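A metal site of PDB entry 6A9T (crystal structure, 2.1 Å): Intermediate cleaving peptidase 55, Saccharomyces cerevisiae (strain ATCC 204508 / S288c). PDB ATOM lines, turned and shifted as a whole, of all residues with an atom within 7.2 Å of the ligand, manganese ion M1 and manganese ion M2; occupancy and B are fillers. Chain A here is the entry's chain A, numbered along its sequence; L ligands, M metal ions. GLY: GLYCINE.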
ATOM      1  N   TYR A 240      10.187  -0.064  20.782  1.00  0.00           N
ATOM      2  CA  TYR A 240      11.168  -1.130  20.641  1.00  0.00           C
ATOM      3  C   TYR A 240      10.419  -2.447  20.559  1.00  0.00           C
ATOM      4  O   TYR A 240       9.204  -2.514  20.783  1.00  0.00           O
ATOM      5  CB  TYR A 240      12.159  -1.123  21.816  1.00  0.00           C
ATOM      6  CG  TYR A 240      11.501  -1.009  23.168  1.00  0.00           C
ATOM      7  CD1 TYR A 240      11.270   0.239  23.741  1.00  0.00           C
ATOM      8  CD2 TYR A 240      11.105  -2.138  23.878  1.00  0.00           C
ATOM      9  CE1 TYR A 240      10.661   0.358  24.977  1.00  0.00           C
ATOM     10  CE2 TYR A 240      10.494  -2.029  25.116  1.00  0.00           C
ATOM     11  CZ  TYR A 240      10.270  -0.776  25.660  1.00  0.00           C
ATOM     12  OH  TYR A 240       9.669  -0.659  26.891  1.00  0.00           O
ATOM     13  N   ILE A 241      11.145  -3.505  20.234  1.00  0.00           N
ATOM     14  CA  ILE A 241      10.582  -4.856  20.192  1.00  0.00           C
ATOM     15  C   ILE A 241      10.217  -5.253  21.620  1.00  0.00           C
ATOM     16  O   ILE A 241      11.080  -5.240  22.508  1.00  0.00           O
ATOM     17  CB  ILE A 241      11.539  -5.863  19.547  1.00  0.00           C
ATOM     18  CG1 ILE A 241      11.736  -5.538  18.066  1.00  0.00           C
ATOM     19  CG2 ILE A 241      11.023  -7.276  19.719  1.00  0.00           C
ATOM     20  CD1 ILE A 241      12.639  -6.493  17.333  1.00  0.00           C
ATOM     21  N   PRO A 242       8.956  -5.593  21.889  1.00  0.00           N
ATOM     22  CA  PRO A 242       8.517  -5.765  23.271  1.00  0.00           C
ATOM     23  C   PRO A 242       8.891  -7.116  23.856  1.00  0.00           C
ATOM     24  O   PRO A 242       9.048  -8.113  23.151  1.00  0.00           O
ATOM     25  CB  PRO A 242       6.987  -5.618  23.164  1.00  0.00           C
ATOM     26  CG  PRO A 242       6.680  -6.146  21.792  1.00  0.00           C
ATOM     27  CD  PRO A 242       7.846  -5.745  20.923  1.00  0.00           C
ATOM     28  N   VAL A 243       9.025  -7.119  25.177  1.00  0.00           N
ATOM     29  CA  VAL A 243       9.242  -8.339  25.944  1.00  0.00           C
ATOM     30  C   VAL A 243       7.954  -8.670  26.670  1.00  0.00           C
ATOM     31  O   VAL A 243       7.432  -7.837  27.423  1.00  0.00           O
ATOM     32  CB  VAL A 243      10.404  -8.180  26.936  1.00  0.00           C
ATOM     33  CG1 VAL A 243      10.551  -9.424  27.811  1.00  0.00           C
ATOM     34  CG2 VAL A 243      11.700  -7.883  26.197  1.00  0.00           C
ATOM     35  N   VAL A 270       6.798  -7.707  31.497  1.00  0.00           N
ATOM     36  CA  VAL A 270       6.494  -7.030  30.243  1.00  0.00           C
ATOM     37  C   VAL A 270       7.354  -5.778  30.141  1.00  0.00           C
ATOM     38  O   VAL A 270       7.300  -4.906  31.019  1.00  0.00           O
ATOM     39  CB  VAL A 270       5.006  -6.688  30.113  1.00  0.00           C
ATOM     40  CG1 VAL A 270       4.773  -5.856  28.858  1.00  0.00           C
ATOM     41  CG2 VAL A 270       4.173  -7.948  30.068  1.00  0.00           C
ATOM     42  N   ASP A 271       8.144  -5.696  29.067  1.00  0.00           N
ATOM     43  CA  ASP A 271       8.911  -4.505  28.721  1.00  0.00           C
ATOM     44  C   ASP A 271       8.403  -4.014  27.377  1.00  0.00           C
ATOM     45  O   ASP A 271       8.718  -4.617  26.341  1.00  0.00           O
ATOM     46  CB  ASP A 271      10.403  -4.804  28.689  1.00  0.00           C
ATOM     47  CG  ASP A 271      11.266  -3.543  28.703  1.00  0.00           C
ATOM     48  OD1 ASP A 271      10.738  -2.466  28.375  1.00  0.00           O
ATOM     49  OD2 ASP A 271      12.460  -3.641  29.045  1.00  0.00           O
ATOM     50  N   ALA A 272       7.614  -2.953  27.385  1.00  0.00           N
ATOM     51  CA  ALA A 272       6.991  -2.458  26.162  1.00  0.00           C
ATOM     52  C   ALA A 272       6.562  -1.016  26.366  1.00  0.00           C
ATOM     53  O   ALA A 272       6.215  -0.612  27.478  1.00  0.00           O
ATOM     54  CB  ALA A 272       5.790  -3.318  25.765  1.00  0.00           C
ATOM     55  N   ALA A 273       6.589  -0.246  25.283  1.00  0.00           N
ATOM     56  CA  ALA A 273       6.195   1.155  25.326  1.00  0.00           C
ATOM     57  C   ALA A 273       6.036   1.663  23.900  1.00  0.00           C
ATOM     58  O   ALA A 273       6.552   1.083  22.948  1.00  0.00           O
ATOM     59  CB  ALA A 273       7.225   2.015  26.083  1.00  0.00           C
ATOM     60  N   ALA A 281       9.192   6.183  24.854  1.00  0.00           N
ATOM     61  CA  ALA A 281       9.027   5.819  26.246  1.00  0.00           C
ATOM     62  C   ALA A 281       9.628   4.425  26.440  1.00  0.00           C
ATOM     63  O   ALA A 281      10.052   3.772  25.482  1.00  0.00           O
ATOM     64  CB  ALA A 281       7.547   5.862  26.642  1.00  0.00           C
ATOM     65  N   ASP A 282       9.666   3.971  27.688  1.00  0.00           N
ATOM     66  CA  ASP A 282      10.291   2.687  27.998  1.00  0.00           C
ATOM     67  C   ASP A 282       9.814   2.231  29.361  1.00  0.00           C
ATOM     68  O   ASP A 282      10.214   2.810  30.382  1.00  0.00           O
ATOM     69  CB  ASP A 282      11.812   2.821  27.952  1.00  0.00           C
ATOM     70  CG  ASP A 282      12.524   1.487  27.974  1.00  0.00           C
ATOM     71  OD1 ASP A 282      11.858   0.452  28.157  1.00  0.00           O
ATOM     72  OD2 ASP A 282      13.766   1.478  27.799  1.00  0.00           O
ATOM     73  N   ILE A 283       8.965   1.211  29.397  1.00  0.00           N
ATOM     74  CA  ILE A 283       8.315   0.773  30.631  1.00  0.00           C
ATOM     75  C   ILE A 283       8.526  -0.722  30.810  1.00  0.00           C
ATOM     76  O   ILE A 283       8.394  -1.505  29.852  1.00  0.00           O
ATOM     77  CB  ILE A 283       6.810   1.108  30.632  1.00  0.00           C
ATOM     78  CG1 ILE A 283       6.597   2.622  30.500  1.00  0.00           C
ATOM     79  CG2 ILE A 283       6.140   0.596  31.898  1.00  0.00           C
ATOM     80  CD1 ILE A 283       5.149   3.027  30.529  1.00  0.00           C
ATOM     81  N   SER A 284       8.834  -1.129  32.035  1.00  0.00           N
ATOM     82  CA  SER A 284       8.811  -2.527  32.438  1.00  0.00           C
ATOM     83  C   SER A 284       7.915  -2.662  33.668  1.00  0.00           C
ATOM     84  O   SER A 284       8.052  -1.901  34.625  1.00  0.00           O
ATOM     85  CB  SER A 284      10.210  -3.060  32.763  1.00  0.00           C
ATOM     86  OG  SER A 284      11.072  -2.944  31.639  1.00  0.00           O
ATOM     87  N   ILE A 359      21.622  -0.224  35.483  1.00  0.00           N
ATOM     88  CA  ILE A 359      20.469   0.380  36.150  1.00  0.00           C
ATOM     89  C   ILE A 359      19.555   1.067  35.142  1.00  0.00           C
ATOM     90  O   ILE A 359      18.346   1.183  35.369  1.00  0.00           O
ATOM     91  CB  ILE A 359      20.931   1.343  37.249  1.00  0.00           C
ATOM     92  CG1 ILE A 359      19.741   1.819  38.095  1.00  0.00           C
ATOM     93  CG2 ILE A 359      21.629   2.558  36.647  1.00  0.00           C
ATOM     94  CD1 ILE A 359      18.896   0.692  38.640  1.00  0.00           C
ATOM     95  N   GLY A 360      20.113   1.548  34.035  1.00  0.00           N
ATOM     96  CA  GLY A 360      19.300   2.283  33.077  1.00  0.00           C
ATOM     97  C   GLY A 360      20.174   2.907  32.003  1.00  0.00           C
ATOM     98  O   GLY A 360      21.315   2.494  31.790  1.00  0.00           O
ATOM     99  N   HIS A 361      19.612   3.908  31.335  1.00  0.00           N
ATOM    100  CA  HIS A 361      20.224   4.481  30.148  1.00  0.00           C
ATOM    101  C   HIS A 361      19.504   5.783  29.814  1.00  0.00           C
ATOM    102  O   HIS A 361      18.354   5.995  30.219  1.00  0.00           O
ATOM    103  CB  HIS A 361      20.139   3.511  28.964  1.00  0.00           C
ATOM    104  CG  HIS A 361      18.760   3.010  28.693  1.00  0.00           C
ATOM    105  ND1 HIS A 361      17.837   3.724  27.950  1.00  0.00           N
ATOM    106  CD2 HIS A 361      18.124   1.885  29.091  1.00  0.00           C
ATOM    107  CE1 HIS A 361      16.716   3.045  27.889  1.00  0.00           C
ATOM    108  NE2 HIS A 361      16.857   1.922  28.577  1.00  0.00           N
ATOM    109  N   ASN A 362      20.193   6.649  29.072  1.00  0.00           N
ATOM    110  CA  ASN A 362      19.537   7.823  28.519  1.00  0.00           C
ATOM    111  C   ASN A 362      18.437   7.405  27.548  1.00  0.00           C
ATOM    112  O   ASN A 362      18.508   6.358  26.915  1.00  0.00           O
ATOM    113  CB  ASN A 362      20.558   8.716  27.801  1.00  0.00           C
ATOM    114  CG  ASN A 362      21.384   9.543  28.763  1.00  0.00           C
ATOM    115  OD1 ASN A 362      20.946  10.602  29.225  1.00  0.00           O
ATOM    116  ND2 ASN A 362      22.590   9.078  29.062  1.00  0.00           N
ATOM    117  N   LEU A 363      17.407   8.252  27.457  1.00  0.00           N
ATOM    118  CA  LEU A 363      16.233   7.943  26.655  1.00  0.00           C
ATOM    119  C   LEU A 363      15.846   9.174  25.840  1.00  0.00           C
ATOM    120  O   LEU A 363      15.828  10.287  26.361  1.00  0.00           O
ATOM    121  CB  LEU A 363      15.059   7.505  27.544  1.00  0.00           C
ATOM    122  CG  LEU A 363      13.763   7.086  26.855  1.00  0.00           C
ATOM    123  CD1 LEU A 363      13.925   5.750  26.144  1.00  0.00           C
ATOM    124  CD2 LEU A 363      12.639   7.021  27.866  1.00  0.00           C
ATOM    125  N   VAL A 367      15.952   4.534  21.904  1.00  0.00           N
ATOM    126  CA  VAL A 367      15.654   3.911  23.193  1.00  0.00           C
ATOM    127  C   VAL A 367      16.881   3.966  24.094  1.00  0.00           C
ATOM    128  O   VAL A 367      16.841   4.500  25.211  1.00  0.00           O
ATOM    129  CB  VAL A 367      15.169   2.464  23.003  1.00  0.00           C
ATOM    130  CG1 VAL A 367      14.781   1.849  24.336  1.00  0.00           C
ATOM    131  CG2 VAL A 367      13.994   2.433  22.042  1.00  0.00           C
ATOM    132  N   HIS A 368      17.995   3.419  23.614  1.00  0.00           N
ATOM    133  CA  HIS A 368      19.289   3.598  24.269  1.00  0.00           C
ATOM    134  C   HIS A 368      19.929   4.852  23.676  1.00  0.00           C
ATOM    135  O   HIS A 368      20.816   4.799  22.827  1.00  0.00           O
ATOM    136  CB  HIS A 368      20.151   2.359  24.113  1.00  0.00           C
ATOM    137  CG  HIS A 368      19.610   1.156  24.829  1.00  0.00           C
ATOM    138  ND1 HIS A 368      20.175  -0.102  24.722  1.00  0.00           N
ATOM    139  CD2 HIS A 368      18.558   1.023  25.670  1.00  0.00           C
ATOM    140  CE1 HIS A 368      19.488  -0.948  25.460  1.00  0.00           C
ATOM    141  NE2 HIS A 368      18.496  -0.295  26.042  1.00  0.00           N
ATOM    142  N   THR A 386      16.360   6.046  32.336  1.00  0.00           N
ATOM    143  CA  THR A 386      15.511   5.015  32.898  1.00  0.00           C
ATOM    144  C   THR A 386      16.121   4.505  34.202  1.00  0.00           C
ATOM    145  O   THR A 386      17.336   4.555  34.408  1.00  0.00           O
ATOM    146  CB  THR A 386      15.342   3.854  31.917  1.00  0.00           C
ATOM    147  OG1 THR A 386      16.602   3.221  31.686  1.00  0.00           O
ATOM    148  CG2 THR A 386      14.778   4.346  30.598  1.00  0.00           C
ATOM    149  N   ILE A 387      15.250   4.033  35.092  1.00  0.00           N
ATOM    150  CA  ILE A 387      15.647   3.362  36.322  1.00  0.00           C
ATOM    151  C   ILE A 387      14.952   2.021  36.315  1.00  0.00           C
ATOM    152  O   ILE A 387      13.731   1.953  36.531  1.00  0.00           O
ATOM    153  CB  ILE A 387      15.283   4.170  37.571  1.00  0.00           C
ATOM    154  CG1 ILE A 387      15.953   5.548  37.543  1.00  0.00           C
ATOM    155  CG2 ILE A 387      15.690   3.420  38.826  1.00  0.00           C
ATOM    156  CD1 ILE A 387      17.459   5.497  37.656  1.00  0.00           C
ATOM    157  N   GLU A 388      15.709   0.942  36.068  1.00  0.00           N
ATOM    158  CA  GLU A 388      15.121  -0.375  35.800  1.00  0.00           C
ATOM    159  C   GLU A 388      15.954  -1.474  36.436  1.00  0.00           C
ATOM    160  O   GLU A 388      16.550  -2.304  35.743  1.00  0.00           O
ATOM    161  CB  GLU A 388      14.984  -0.586  34.300  1.00  0.00           C
ATOM    162  CG  GLU A 388      16.221  -0.213  33.495  1.00  0.00           C
ATOM    163  CD  GLU A 388      16.079  -0.560  32.036  1.00  0.00           C
ATOM    164  OE1 GLU A 388      16.478   0.269  31.186  1.00  0.00           O
ATOM    165  OE2 GLU A 388      15.552  -1.655  31.730  1.00  0.00           O
ATOM    166  N   ARG A 409      11.297  -7.052  36.702  1.00  0.00           N
ATOM    167  CA  ARG A 409      11.897  -5.766  36.382  1.00  0.00           C
ATOM    168  C   ARG A 409      10.822  -4.690  36.463  1.00  0.00           C
ATOM    169  O   ARG A 409       9.689  -4.898  36.041  1.00  0.00           O
ATOM    170  CB  ARG A 409      12.551  -5.753  34.997  1.00  0.00           C
ATOM    171  CG  ARG A 409      13.247  -4.436  34.684  1.00  0.00           C
ATOM    172  CD  ARG A 409      14.265  -4.551  33.566  1.00  0.00           C
ATOM    173  NE  ARG A 409      13.658  -4.787  32.263  1.00  0.00           N
ATOM    174  CZ  ARG A 409      13.673  -5.958  31.642  1.00  0.00           C
ATOM    175  NH1 ARG A 409      14.274  -7.004  32.194  1.00  0.00           N
ATOM    176  NH2 ARG A 409      13.090  -6.095  30.456  1.00  0.00           N
ATOM    177  N   GLU A 411      10.552  -0.614  35.519  1.00  0.00           N
ATOM    178  CA  GLU A 411      11.245   0.438  34.793  1.00  0.00           C
ATOM    179  C   GLU A 411      10.359   1.667  34.643  1.00  0.00           C
ATOM    180  O   GLU A 411       9.183   1.551  34.311  1.00  0.00           O
ATOM    181  CB  GLU A 411      11.681  -0.045  33.406  1.00  0.00           C
ATOM    182  CG  GLU A 411      12.321   1.019  32.534  1.00  0.00           C
ATOM    183  CD  GLU A 411      12.899   0.446  31.255  1.00  0.00           C
ATOM    184  OE1 GLU A 411      12.458  -0.647  30.835  1.00  0.00           O
ATOM    185  OE2 GLU A 411      13.796   1.082  30.678  1.00  0.00           O
ATOM    186  N   ASP A 412      10.944   2.836  34.881  1.00  0.00           N
ATOM    187  CA  ASP A 412      10.272   4.113  34.673  1.00  0.00           C
ATOM    188  C   ASP A 412      11.246   5.084  34.025  1.00  0.00           C
ATOM    189  O   ASP A 412      12.464   4.904  34.085  1.00  0.00           O
ATOM    190  CB  ASP A 412       9.734   4.688  35.997  1.00  0.00           C
ATOM    191  CG  ASP A 412       8.501   3.954  36.489  1.00  0.00           C
ATOM    192  OD1 ASP A 412       7.418   4.116  35.880  1.00  0.00           O
ATOM    193  OD2 ASP A 412       8.606   3.192  37.474  1.00  0.00           O
ATOM    194  N   ASP A 413      10.690   6.112  33.397  1.00  0.00           N
ATOM    195  CA  ASP A 413      11.465   7.126  32.682  1.00  0.00           C
ATOM    196  C   ASP A 413      11.491   8.392  33.530  1.00  0.00           C
ATOM    197  O   ASP A 413      10.438   8.972  33.825  1.00  0.00           O
ATOM    198  CB  ASP A 413      10.867   7.388  31.312  1.00  0.00           C
ATOM    199  CG  ASP A 413      10.685   6.116  30.505  1.00  0.00           C
ATOM    200  OD1 ASP A 413      11.426   5.157  30.769  1.00  0.00           O
ATOM    201  OD2 ASP A 413       9.806   6.084  29.617  1.00  0.00           O
HETATM  202  N   GLY L   1      13.489  -1.735  26.506  1.00  0.00           N
HETATM  203  CA  GLY L   1      14.904  -2.009  26.688  1.00  0.00           C
HETATM  204  C   GLY L   1      15.448  -1.459  27.989  1.00  0.00           C
HETATM  205  O   GLY L   1      16.453  -0.757  27.991  1.00  0.00           O
HETATM  206  OXT GLY L   1      14.907  -1.713  29.063  1.00  0.00           O
HETATM  207 MN    MN M   1      15.221   0.534  29.213  1.00  0.00          MN
HETATM  208 MN    MN M   2      12.686  -1.398  28.822  1.00  0.00          MN
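Residues that only touch the ligand: Tyr 240 (3.3 Å).
Hydrophobic or aromatic side chains that line the ligand: Tyr 240, His 361 and His 368.
An oxygen (O) of the ligand lies close to a ring nitrogen (NE2) of His 368 (2.9 Å).
Manganese ion M2 is bound by the side-chain carboxylate (OD1) of Asp 282 (2.1 Å), the side-chain carboxylate (OE1) of Glu 411 (2.2 Å), an oxygen (OXT) of the ligand (2.3 Å), the side-chain carboxylate (OD2) of Asp 271 (2.3 Å), the side-chain carboxylate (OD1) of Asp 271 (2.3 Å) and a nitrogen (N) of the ligand (2.5 Å).
Thr 386 touches manganese ion M1.
The nearest printed residue that does not touch manganese ion M1 is His 368 (4.6 Å).
Manganese ion M1 is bound by the side-chain carboxylate (OE2) of Glu 411, at 2.1 Å.
Manganese ion M1 is bound by O of the ligand (2.2 Å).
OD2 of Asp 282 is bound to manganese ion M1 (2.2 Å).
A ring nitrogen (NE2) of His 361 is bound to manganese ion M1 (2.2 Å).
OXT of the ligand binds manganese ion M1, at 2.3 Å.
OE1 of Glu 388 binds manganese ion M1, at 2.4 Å.
Manganese ion M1 has six donor atoms within binding distance.
OH of Tyr 240 sits close to OD1 of Asp 282.
N of Thr 386 sits at hydrogen-bond distance from O of His 361 (2.9 Å).
ND1 of His 361 lies within hydrogen-bond range of O of Val 367.
The side-chain carboxylate (OD2) of Asp 271 sits close to the guanidinium group (NH2) of Arg 409 (2.9 Å).
O of Asp 271 is in hydrogen-bond range of N of Val 243, at 2.8 Å.
OE2 of Glu 388 lies within salt-bridge range of NE of Arg 409, 3.7 Å away.
N of Ile 283 lies within hydrogen-bond range of OH of Tyr 240, at 3.2 Å.
OH of Tyr 240 is in hydrogen-bond range of N of Ala 272.
Tyr 240 touches manganese ion M2 (OH to MN, 3.7 Å).
Ser 284 touches manganese ion M2.
Of the 26 residues printed, 5 come within 4 Å of manganese ion M2.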
